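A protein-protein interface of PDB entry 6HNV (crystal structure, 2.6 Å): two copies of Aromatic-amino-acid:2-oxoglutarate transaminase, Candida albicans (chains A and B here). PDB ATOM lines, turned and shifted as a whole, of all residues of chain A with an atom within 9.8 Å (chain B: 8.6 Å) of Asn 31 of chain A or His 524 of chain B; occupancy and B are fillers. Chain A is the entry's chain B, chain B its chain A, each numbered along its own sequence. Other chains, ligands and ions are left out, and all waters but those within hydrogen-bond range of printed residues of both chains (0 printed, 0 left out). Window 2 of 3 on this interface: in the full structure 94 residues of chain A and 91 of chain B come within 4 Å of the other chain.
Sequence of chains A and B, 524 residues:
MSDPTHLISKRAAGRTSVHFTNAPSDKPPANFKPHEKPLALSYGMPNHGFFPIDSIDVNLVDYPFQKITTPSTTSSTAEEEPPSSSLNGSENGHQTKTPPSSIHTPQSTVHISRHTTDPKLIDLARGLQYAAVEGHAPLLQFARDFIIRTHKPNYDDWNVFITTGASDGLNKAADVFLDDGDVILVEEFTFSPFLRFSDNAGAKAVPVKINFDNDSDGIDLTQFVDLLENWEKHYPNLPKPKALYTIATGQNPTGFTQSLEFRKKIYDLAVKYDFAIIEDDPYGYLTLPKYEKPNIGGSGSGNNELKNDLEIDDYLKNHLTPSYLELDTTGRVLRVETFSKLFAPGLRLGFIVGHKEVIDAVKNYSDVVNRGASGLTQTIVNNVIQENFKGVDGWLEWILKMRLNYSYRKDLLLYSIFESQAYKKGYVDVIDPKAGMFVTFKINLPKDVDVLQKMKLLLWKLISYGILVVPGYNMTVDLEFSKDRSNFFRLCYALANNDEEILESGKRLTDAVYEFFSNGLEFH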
ATOM      1  N   LYS A  27     -30.002   4.647   1.148  1.00  0.00           N
ATOM      2  CA  LYS A  27     -29.979   3.168   1.020  1.00  0.00           C
ATOM      3  C   LYS A  27     -28.738   2.818   0.200  1.00  0.00           C
ATOM      4  O   LYS A  27     -28.564   3.343  -0.905  1.00  0.00           O
ATOM      5  CB  LYS A  27     -31.262   2.624   0.370  1.00  0.00           C
ATOM      6  CG  LYS A  27     -31.786   1.307   0.949  1.00  0.00           C
ATOM      7  CD  LYS A  27     -32.061   0.204  -0.074  1.00  0.00           C
ATOM      8  CE  LYS A  27     -33.066   0.580  -1.143  1.00  0.00           C
ATOM      9  NZ  LYS A  27     -33.339  -0.555  -2.057  1.00  0.00           N
ATOM     10  N   PRO A  28     -27.832   1.959   0.728  1.00  0.00           N
ATOM     11  CA  PRO A  28     -26.724   1.428  -0.064  1.00  0.00           C
ATOM     12  C   PRO A  28     -27.212   0.434  -1.111  1.00  0.00           C
ATOM     13  O   PRO A  28     -28.327  -0.073  -1.002  1.00  0.00           O
ATOM     14  CB  PRO A  28     -25.847   0.716   0.969  1.00  0.00           C
ATOM     15  CG  PRO A  28     -26.814   0.328   2.059  1.00  0.00           C
ATOM     16  CD  PRO A  28     -27.819   1.457   2.109  1.00  0.00           C
ATOM     17  N   PRO A  29     -26.395   0.100  -2.140  1.00  0.00           N
ATOM     18  CA  PRO A  29     -26.789  -0.881  -3.152  1.00  0.00           C
ATOM     19  C   PRO A  29     -26.996  -2.265  -2.520  1.00  0.00           C
ATOM     20  O   PRO A  29     -26.404  -2.539  -1.475  1.00  0.00           O
ATOM     21  CB  PRO A  29     -25.624  -0.926  -4.153  1.00  0.00           C
ATOM     22  CG  PRO A  29     -24.801   0.311  -3.841  1.00  0.00           C
ATOM     23  CD  PRO A  29     -25.042   0.624  -2.377  1.00  0.00           C
ATOM     24  N   ALA A  30     -27.809  -3.093  -3.181  1.00  0.00           N
ATOM     25  CA  ALA A  30     -28.324  -4.393  -2.681  1.00  0.00           C
ATOM     26  C   ALA A  30     -27.195  -5.302  -2.155  1.00  0.00           C
ATOM     27  O   ALA A  30     -27.421  -5.986  -1.123  1.00  0.00           O
ATOM     28  CB  ALA A  30     -29.114  -5.065  -3.781  1.00  0.00           C
ATOM     29  N   ASN A  31     -26.033  -5.334  -2.819  1.00  0.00           N
ATOM     30  CA  ASN A  31     -24.983  -6.363  -2.579  1.00  0.00           C
ATOM     31  C   ASN A  31     -23.759  -5.729  -1.908  1.00  0.00           C
ATOM     32  O   ASN A  31     -22.627  -6.011  -2.339  1.00  0.00           O
ATOM     33  CB  ASN A  31     -24.647  -7.117  -3.870  1.00  0.00           C
ATOM     34  CG  ASN A  31     -24.987  -8.589  -3.772  1.00  0.00           C
ATOM     35  OD1 ASN A  31     -24.764  -9.209  -2.734  1.00  0.00           O
ATOM     36  ND2 ASN A  31     -25.519  -9.155  -4.841  1.00  0.00           N
ATOM     37  N   PHE A  32     -23.985  -4.956  -0.850  1.00  0.00           N
ATOM     38  CA  PHE A  32     -22.950  -4.133  -0.183  1.00  0.00           C
ATOM     39  C   PHE A  32     -22.823  -4.575   1.283  1.00  0.00           C
ATOM     40  O   PHE A  32     -23.842  -4.717   1.990  1.00  0.00           O
ATOM     41  CB  PHE A  32     -23.283  -2.642  -0.348  1.00  0.00           C
ATOM     42  CG  PHE A  32     -22.592  -1.726   0.633  1.00  0.00           C
ATOM     43  CD1 PHE A  32     -21.252  -1.409   0.485  1.00  0.00           C
ATOM     44  CD2 PHE A  32     -23.270  -1.218   1.729  1.00  0.00           C
ATOM     45  CE1 PHE A  32     -20.605  -0.597   1.403  1.00  0.00           C
ATOM     46  CE2 PHE A  32     -22.628  -0.397   2.642  1.00  0.00           C
ATOM     47  CZ  PHE A  32     -21.294  -0.092   2.478  1.00  0.00           C
ATOM     48  N   LYS A  33     -21.583  -4.821   1.711  1.00  0.00           N
ATOM     49  CA  LYS A  33     -21.189  -4.967   3.133  1.00  0.00           C
ATOM     50  C   LYS A  33     -19.946  -4.114   3.337  1.00  0.00           C
ATOM     51  O   LYS A  33     -19.059  -4.086   2.485  1.00  0.00           O
ATOM     52  CB  LYS A  33     -20.923  -6.429   3.515  1.00  0.00           C
ATOM     53  CG  LYS A  33     -21.018  -6.720   5.010  1.00  0.00           C
ATOM     54  CD  LYS A  33     -21.056  -8.201   5.379  1.00  0.00           C
ATOM     55  CE  LYS A  33     -21.675  -8.452   6.743  1.00  0.00           C
ATOM     56  NZ  LYS A  33     -21.103  -9.648   7.402  1.00  0.00           N
ATOM     57  N   PRO A  34     -19.844  -3.379   4.465  1.00  0.00           N
ATOM     58  CA  PRO A  34     -18.638  -2.613   4.760  1.00  0.00           C
ATOM     59  C   PRO A  34     -17.442  -3.559   4.914  1.00  0.00           C
ATOM     60  O   PRO A  34     -17.623  -4.688   5.307  1.00  0.00           O
ATOM     61  CB  PRO A  34     -18.964  -1.881   6.073  1.00  0.00           C
ATOM     62  CG  PRO A  34     -20.087  -2.690   6.694  1.00  0.00           C
ATOM     63  CD  PRO A  34     -20.859  -3.265   5.525  1.00  0.00           C
ATOM     64  N   LEU B 457     -22.538   5.951  -6.116  1.00  0.00           N
ATOM     65  CA  LEU B 457     -22.362   4.500  -6.385  1.00  0.00           C
ATOM     66  C   LEU B 457     -20.887   4.131  -6.148  1.00  0.00           C
ATOM     67  O   LEU B 457     -20.629   3.408  -5.174  1.00  0.00           O
ATOM     68  CB  LEU B 457     -22.826   4.199  -7.816  1.00  0.00           C
ATOM     69  CG  LEU B 457     -23.491   2.844  -8.046  1.00  0.00           C
ATOM     70  CD1 LEU B 457     -24.482   2.505  -6.939  1.00  0.00           C
ATOM     71  CD2 LEU B 457     -24.188   2.827  -9.400  1.00  0.00           C
ATOM     72  N   TRP B 460     -19.719   4.145  -2.567  1.00  0.00           N
ATOM     73  CA  TRP B 460     -20.196   2.879  -1.950  1.00  0.00           C
ATOM     74  C   TRP B 460     -19.192   1.766  -2.258  1.00  0.00           C
ATOM     75  O   TRP B 460     -18.875   1.031  -1.331  1.00  0.00           O
ATOM     76  CB  TRP B 460     -21.606   2.500  -2.425  1.00  0.00           C
ATOM     77  CG  TRP B 460     -22.689   3.207  -1.680  1.00  0.00           C
ATOM     78  CD1 TRP B 460     -23.686   3.986  -2.196  1.00  0.00           C
ATOM     79  CD2 TRP B 460     -22.866   3.202  -0.259  1.00  0.00           C
ATOM     80  NE1 TRP B 460     -24.480   4.455  -1.189  1.00  0.00           N
ATOM     81  CE2 TRP B 460     -24.005   3.987   0.010  1.00  0.00           C
ATOM     82  CE3 TRP B 460     -22.180   2.613   0.802  1.00  0.00           C
ATOM     83  CZ2 TRP B 460     -24.466   4.198   1.310  1.00  0.00           C
ATOM     84  CZ3 TRP B 460     -22.638   2.821   2.087  1.00  0.00           C
ATOM     85  CH2 TRP B 460     -23.765   3.604   2.337  1.00  0.00           C
ATOM     86  N   LYS B 461     -18.702   1.675  -3.506  1.00  0.00           N
ATOM     87  CA  LYS B 461     -17.743   0.621  -3.936  1.00  0.00           C
ATOM     88  C   LYS B 461     -16.410   0.865  -3.231  1.00  0.00           C
ATOM     89  O   LYS B 461     -15.861  -0.122  -2.734  1.00  0.00           O
ATOM     90  CB  LYS B 461     -17.571   0.579  -5.457  1.00  0.00           C
ATOM     91  CG  LYS B 461     -17.019  -0.732  -6.009  1.00  0.00           C
ATOM     92  CD  LYS B 461     -18.010  -1.889  -5.959  1.00  0.00           C
ATOM     93  CE  LYS B 461     -17.370  -3.256  -6.104  1.00  0.00           C
ATOM     94  NZ  LYS B 461     -18.050  -4.272  -5.262  1.00  0.00           N
ATOM     95  N   SER B 464     -16.795  -0.459   0.357  1.00  0.00           N
ATOM     96  CA  SER B 464     -16.881  -1.947   0.352  1.00  0.00           C
ATOM     97  C   SER B 464     -15.499  -2.571   0.144  1.00  0.00           C
ATOM     98  O   SER B 464     -15.272  -3.673   0.665  1.00  0.00           O
ATOM     99  CB  SER B 464     -17.862  -2.450  -0.692  1.00  0.00           C
ATOM    100  OG  SER B 464     -17.230  -2.644  -1.944  1.00  0.00           O
ATOM    101  N   GLU B 515     -12.707  -2.290 -10.873  1.00  0.00           N
ATOM    102  CA  GLU B 515     -13.864  -3.211 -10.694  1.00  0.00           C
ATOM    103  C   GLU B 515     -15.161  -2.489 -11.104  1.00  0.00           C
ATOM    104  O   GLU B 515     -15.881  -3.048 -11.947  1.00  0.00           O
ATOM    105  CB  GLU B 515     -13.967  -3.750  -9.264  1.00  0.00           C
ATOM    106  CG  GLU B 515     -14.620  -5.126  -9.187  1.00  0.00           C
ATOM    107  CD  GLU B 515     -15.562  -5.357  -8.011  1.00  0.00           C
ATOM    108  OE1 GLU B 515     -16.761  -5.666  -8.257  1.00  0.00           O
ATOM    109  OE2 GLU B 515     -15.103  -5.238  -6.851  1.00  0.00           O
ATOM    110  N   PHE B 516     -15.442  -1.292 -10.558  1.00  0.00           N
ATOM    111  CA  PHE B 516     -16.682  -0.506 -10.825  1.00  0.00           C
ATOM    112  C   PHE B 516     -16.794  -0.261 -12.323  1.00  0.00           C
ATOM    113  O   PHE B 516     -17.917  -0.340 -12.865  1.00  0.00           O
ATOM    114  CB  PHE B 516     -16.684   0.834 -10.081  1.00  0.00           C
ATOM    115  CG  PHE B 516     -17.832   1.771 -10.385  1.00  0.00           C
ATOM    116  CD1 PHE B 516     -19.053   1.630  -9.747  1.00  0.00           C
ATOM    117  CD2 PHE B 516     -17.668   2.837 -11.257  1.00  0.00           C
ATOM    118  CE1 PHE B 516     -20.097   2.506 -10.005  1.00  0.00           C
ATOM    119  CE2 PHE B 516     -18.710   3.713 -11.516  1.00  0.00           C
ATOM    120  CZ  PHE B 516     -19.924   3.547 -10.887  1.00  0.00           C
ATOM    121  N   SER B 518     -15.097  -2.072 -14.678  1.00  0.00           N
ATOM    122  CA  SER B 518     -15.189  -3.454 -15.227  1.00  0.00           C
ATOM    123  C   SER B 518     -16.628  -3.984 -15.118  1.00  0.00           C
ATOM    124  O   SER B 518     -17.026  -4.792 -15.996  1.00  0.00           O
ATOM    125  CB  SER B 518     -14.203  -4.368 -14.547  1.00  0.00           C
ATOM    126  OG  SER B 518     -12.888  -3.911 -14.805  1.00  0.00           O
ATOM    127  N   ASN B 519     -17.378  -3.532 -14.103  1.00  0.00           N
ATOM    128  CA  ASN B 519     -18.794  -3.918 -13.860  1.00  0.00           C
ATOM    129  C   ASN B 519     -19.741  -3.088 -14.755  1.00  0.00           C
ATOM    130  O   ASN B 519     -20.904  -3.495 -14.887  1.00  0.00           O
ATOM    131  CB  ASN B 519     -19.146  -3.843 -12.368  1.00  0.00           C
ATOM    132  CG  ASN B 519     -18.558  -4.980 -11.553  1.00  0.00           C
ATOM    133  OD1 ASN B 519     -18.357  -6.085 -12.060  1.00  0.00           O
ATOM    134  ND2 ASN B 519     -18.305  -4.739 -10.274  1.00  0.00           N
ATOM    135  N   GLY B 520     -19.273  -1.997 -15.376  1.00  0.00           N
ATOM    136  CA  GLY B 520     -20.071  -1.139 -16.283  1.00  0.00           C
ATOM    137  C   GLY B 520     -20.626   0.095 -15.584  1.00  0.00           C
ATOM    138  O   GLY B 520     -21.626   0.637 -16.076  1.00  0.00           O
ATOM    139  N   LEU B 521     -19.954   0.548 -14.514  1.00  0.00           N
ATOM    140  CA  LEU B 521     -20.360   1.668 -13.627  1.00  0.00           C
ATOM    141  C   LEU B 521     -21.624   1.262 -12.861  1.00  0.00           C
ATOM    142  O   LEU B 521     -22.567   2.076 -12.792  1.00  0.00           O
ATOM    143  CB  LEU B 521     -20.561   2.943 -14.452  1.00  0.00           C
ATOM    144  CG  LEU B 521     -19.480   3.216 -15.491  1.00  0.00           C
ATOM    145  CD1 LEU B 521     -19.784   4.480 -16.267  1.00  0.00           C
ATOM    146  CD2 LEU B 521     -18.109   3.299 -14.840  1.00  0.00           C
ATOM    147  N   GLU B 522     -21.627   0.032 -12.334  1.00  0.00           N
ATOM    148  CA  GLU B 522     -22.607  -0.508 -11.340  1.00  0.00           C
ATOM    149  C   GLU B 522     -21.781  -1.210 -10.235  1.00  0.00           C
ATOM    150  O   GLU B 522     -20.532  -1.163 -10.339  1.00  0.00           O
ATOM    151  CB  GLU B 522     -23.654  -1.426 -12.009  1.00  0.00           C
ATOM    152  CG  GLU B 522     -24.389  -0.859 -13.240  1.00  0.00           C
ATOM    153  CD  GLU B 522     -25.573   0.086 -13.034  1.00  0.00           C
ATOM    154  OE1 GLU B 522     -25.994   0.290 -11.873  1.00  0.00           O
ATOM    155  OE2 GLU B 522     -26.083   0.626 -14.053  1.00  0.00           O
ATOM    156  N   PHE B 523     -22.422  -1.842  -9.233  1.00  0.00           N
ATOM    157  CA  PHE B 523     -21.773  -2.418  -8.014  1.00  0.00           C
ATOM    158  C   PHE B 523     -21.375  -3.899  -8.207  1.00  0.00           C
ATOM    159  O   PHE B 523     -20.219  -4.206  -7.859  1.00  0.00           O
ATOM    160  CB  PHE B 523     -22.669  -2.228  -6.785  1.00  0.00           C
ATOM    161  CG  PHE B 523     -21.967  -2.403  -5.460  1.00  0.00           C
ATOM    162  CD1 PHE B 523     -21.714  -3.666  -4.945  1.00  0.00           C
ATOM    163  CD2 PHE B 523     -21.559  -1.299  -4.720  1.00  0.00           C
ATOM    164  CE1 PHE B 523     -21.064  -3.818  -3.731  1.00  0.00           C
ATOM    165  CE2 PHE B 523     -20.918  -1.454  -3.501  1.00  0.00           C
ATOM    166  CZ  PHE B 523     -20.672  -2.713  -3.011  1.00  0.00           C
ATOM    167  N   HIS B 524     -22.273  -4.774  -8.702  1.00  0.00           N
ATOM    168  CA  HIS B 524     -22.055  -6.228  -8.988  1.00  0.00           C
ATOM    169  C   HIS B 524     -21.571  -6.948  -7.721  1.00  0.00           C
ATOM    170  O   HIS B 524     -22.304  -7.159  -6.747  1.00  0.00           O
ATOM    171  CB  HIS B 524     -21.074  -6.439 -10.162  1.00  0.00           C
ATOM    172  CG  HIS B 524     -21.249  -7.707 -10.948  1.00  0.00           C
ATOM    173  ND1 HIS B 524     -20.770  -8.931 -10.513  1.00  0.00           N
ATOM    174  CD2 HIS B 524     -21.795  -7.933 -12.166  1.00  0.00           C
ATOM    175  CE1 HIS B 524     -21.045  -9.855 -11.414  1.00  0.00           C
ATOM    176  NE2 HIS B 524     -21.673  -9.267 -12.439  1.00  0.00           N
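NZ of Lys 461 of chain B lies within hydrogen-bond range of O of Phe 523 of chain B.
O of Lys 461 of chain B is in hydrogen-bond range of OG of Ser 464 of chain B, 3.0 Å away.
The side-chain amide nitrogen (ND2) of Asn 519 of chain B is in hydrogen-bond range of the backbone carbonyl oxygen (O) of Phe 523 of chain B.
Among the printed residues, merely in contact across the chains: Pro 28 of chain A with Trp 460 of chain B (3.7 Å), Pro 29 of chain A with Leu 457 of chain B (3.8 Å), Pro 29 of chain A with Trp 460 of chain B (3.6 Å), Pro 29 of chain A with Phe 523 of chain B (3.7 Å), Asn 31 of chain A with Phe 523 of chain B (3.0 Å), Asn 31 of chain A with His 524 of chain B (3.7 Å), Phe 32 of chain A with Trp 460 of chain B (3.2 Å), Phe 32 of chain A with Ser 464 of chain B (3.7 Å), Phe 32 of chain A with Phe 523 of chain B (3.7 Å) and Lys 33 of chain A with Ser 464 of chain B (3.7 Å).
Asn 31 of chain A touches just these residues of chain B: Phe 523 and His 524.
Of the printed residues of chain A, His 524 of chain B touches Asn 31.
Printed residues of chain B within 4 Å of Pro 29 of chain A: Leu 457 (3.8 Å), Trp 460 (3.6 Å) and Phe 523 (3.7 Å).
Of the printed residues of chain A, Ser 464 of chain B touches Phe 32 (3.7 Å) and Lys 33 (3.7 Å).
Gly 520 of chain B touches none of the printed residues of chain A.
The nearest residue of chain B that does not touch Asn 31 of chain A is Lys 461 of chain B (5.7 Å).
Hydrophobic or aromatic side chains of chain A within 4 Å of the printed part of chain B: Pro 28, Pro 29 and Phe 32.
Of the 13 printed residues of chain B, 5 touch a printed residue of chain A.
Printed residues of chain B that touch a printed residue of chain A: Leu 457, Trp 460, Ser 464, Phe 523 and His 524.
Along chain B the printed residues that touch a printed residue of chain A span positions 457 to 524.
Among the printed residues, 10 pairs touch across the chains.
No position is printed for both chains.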
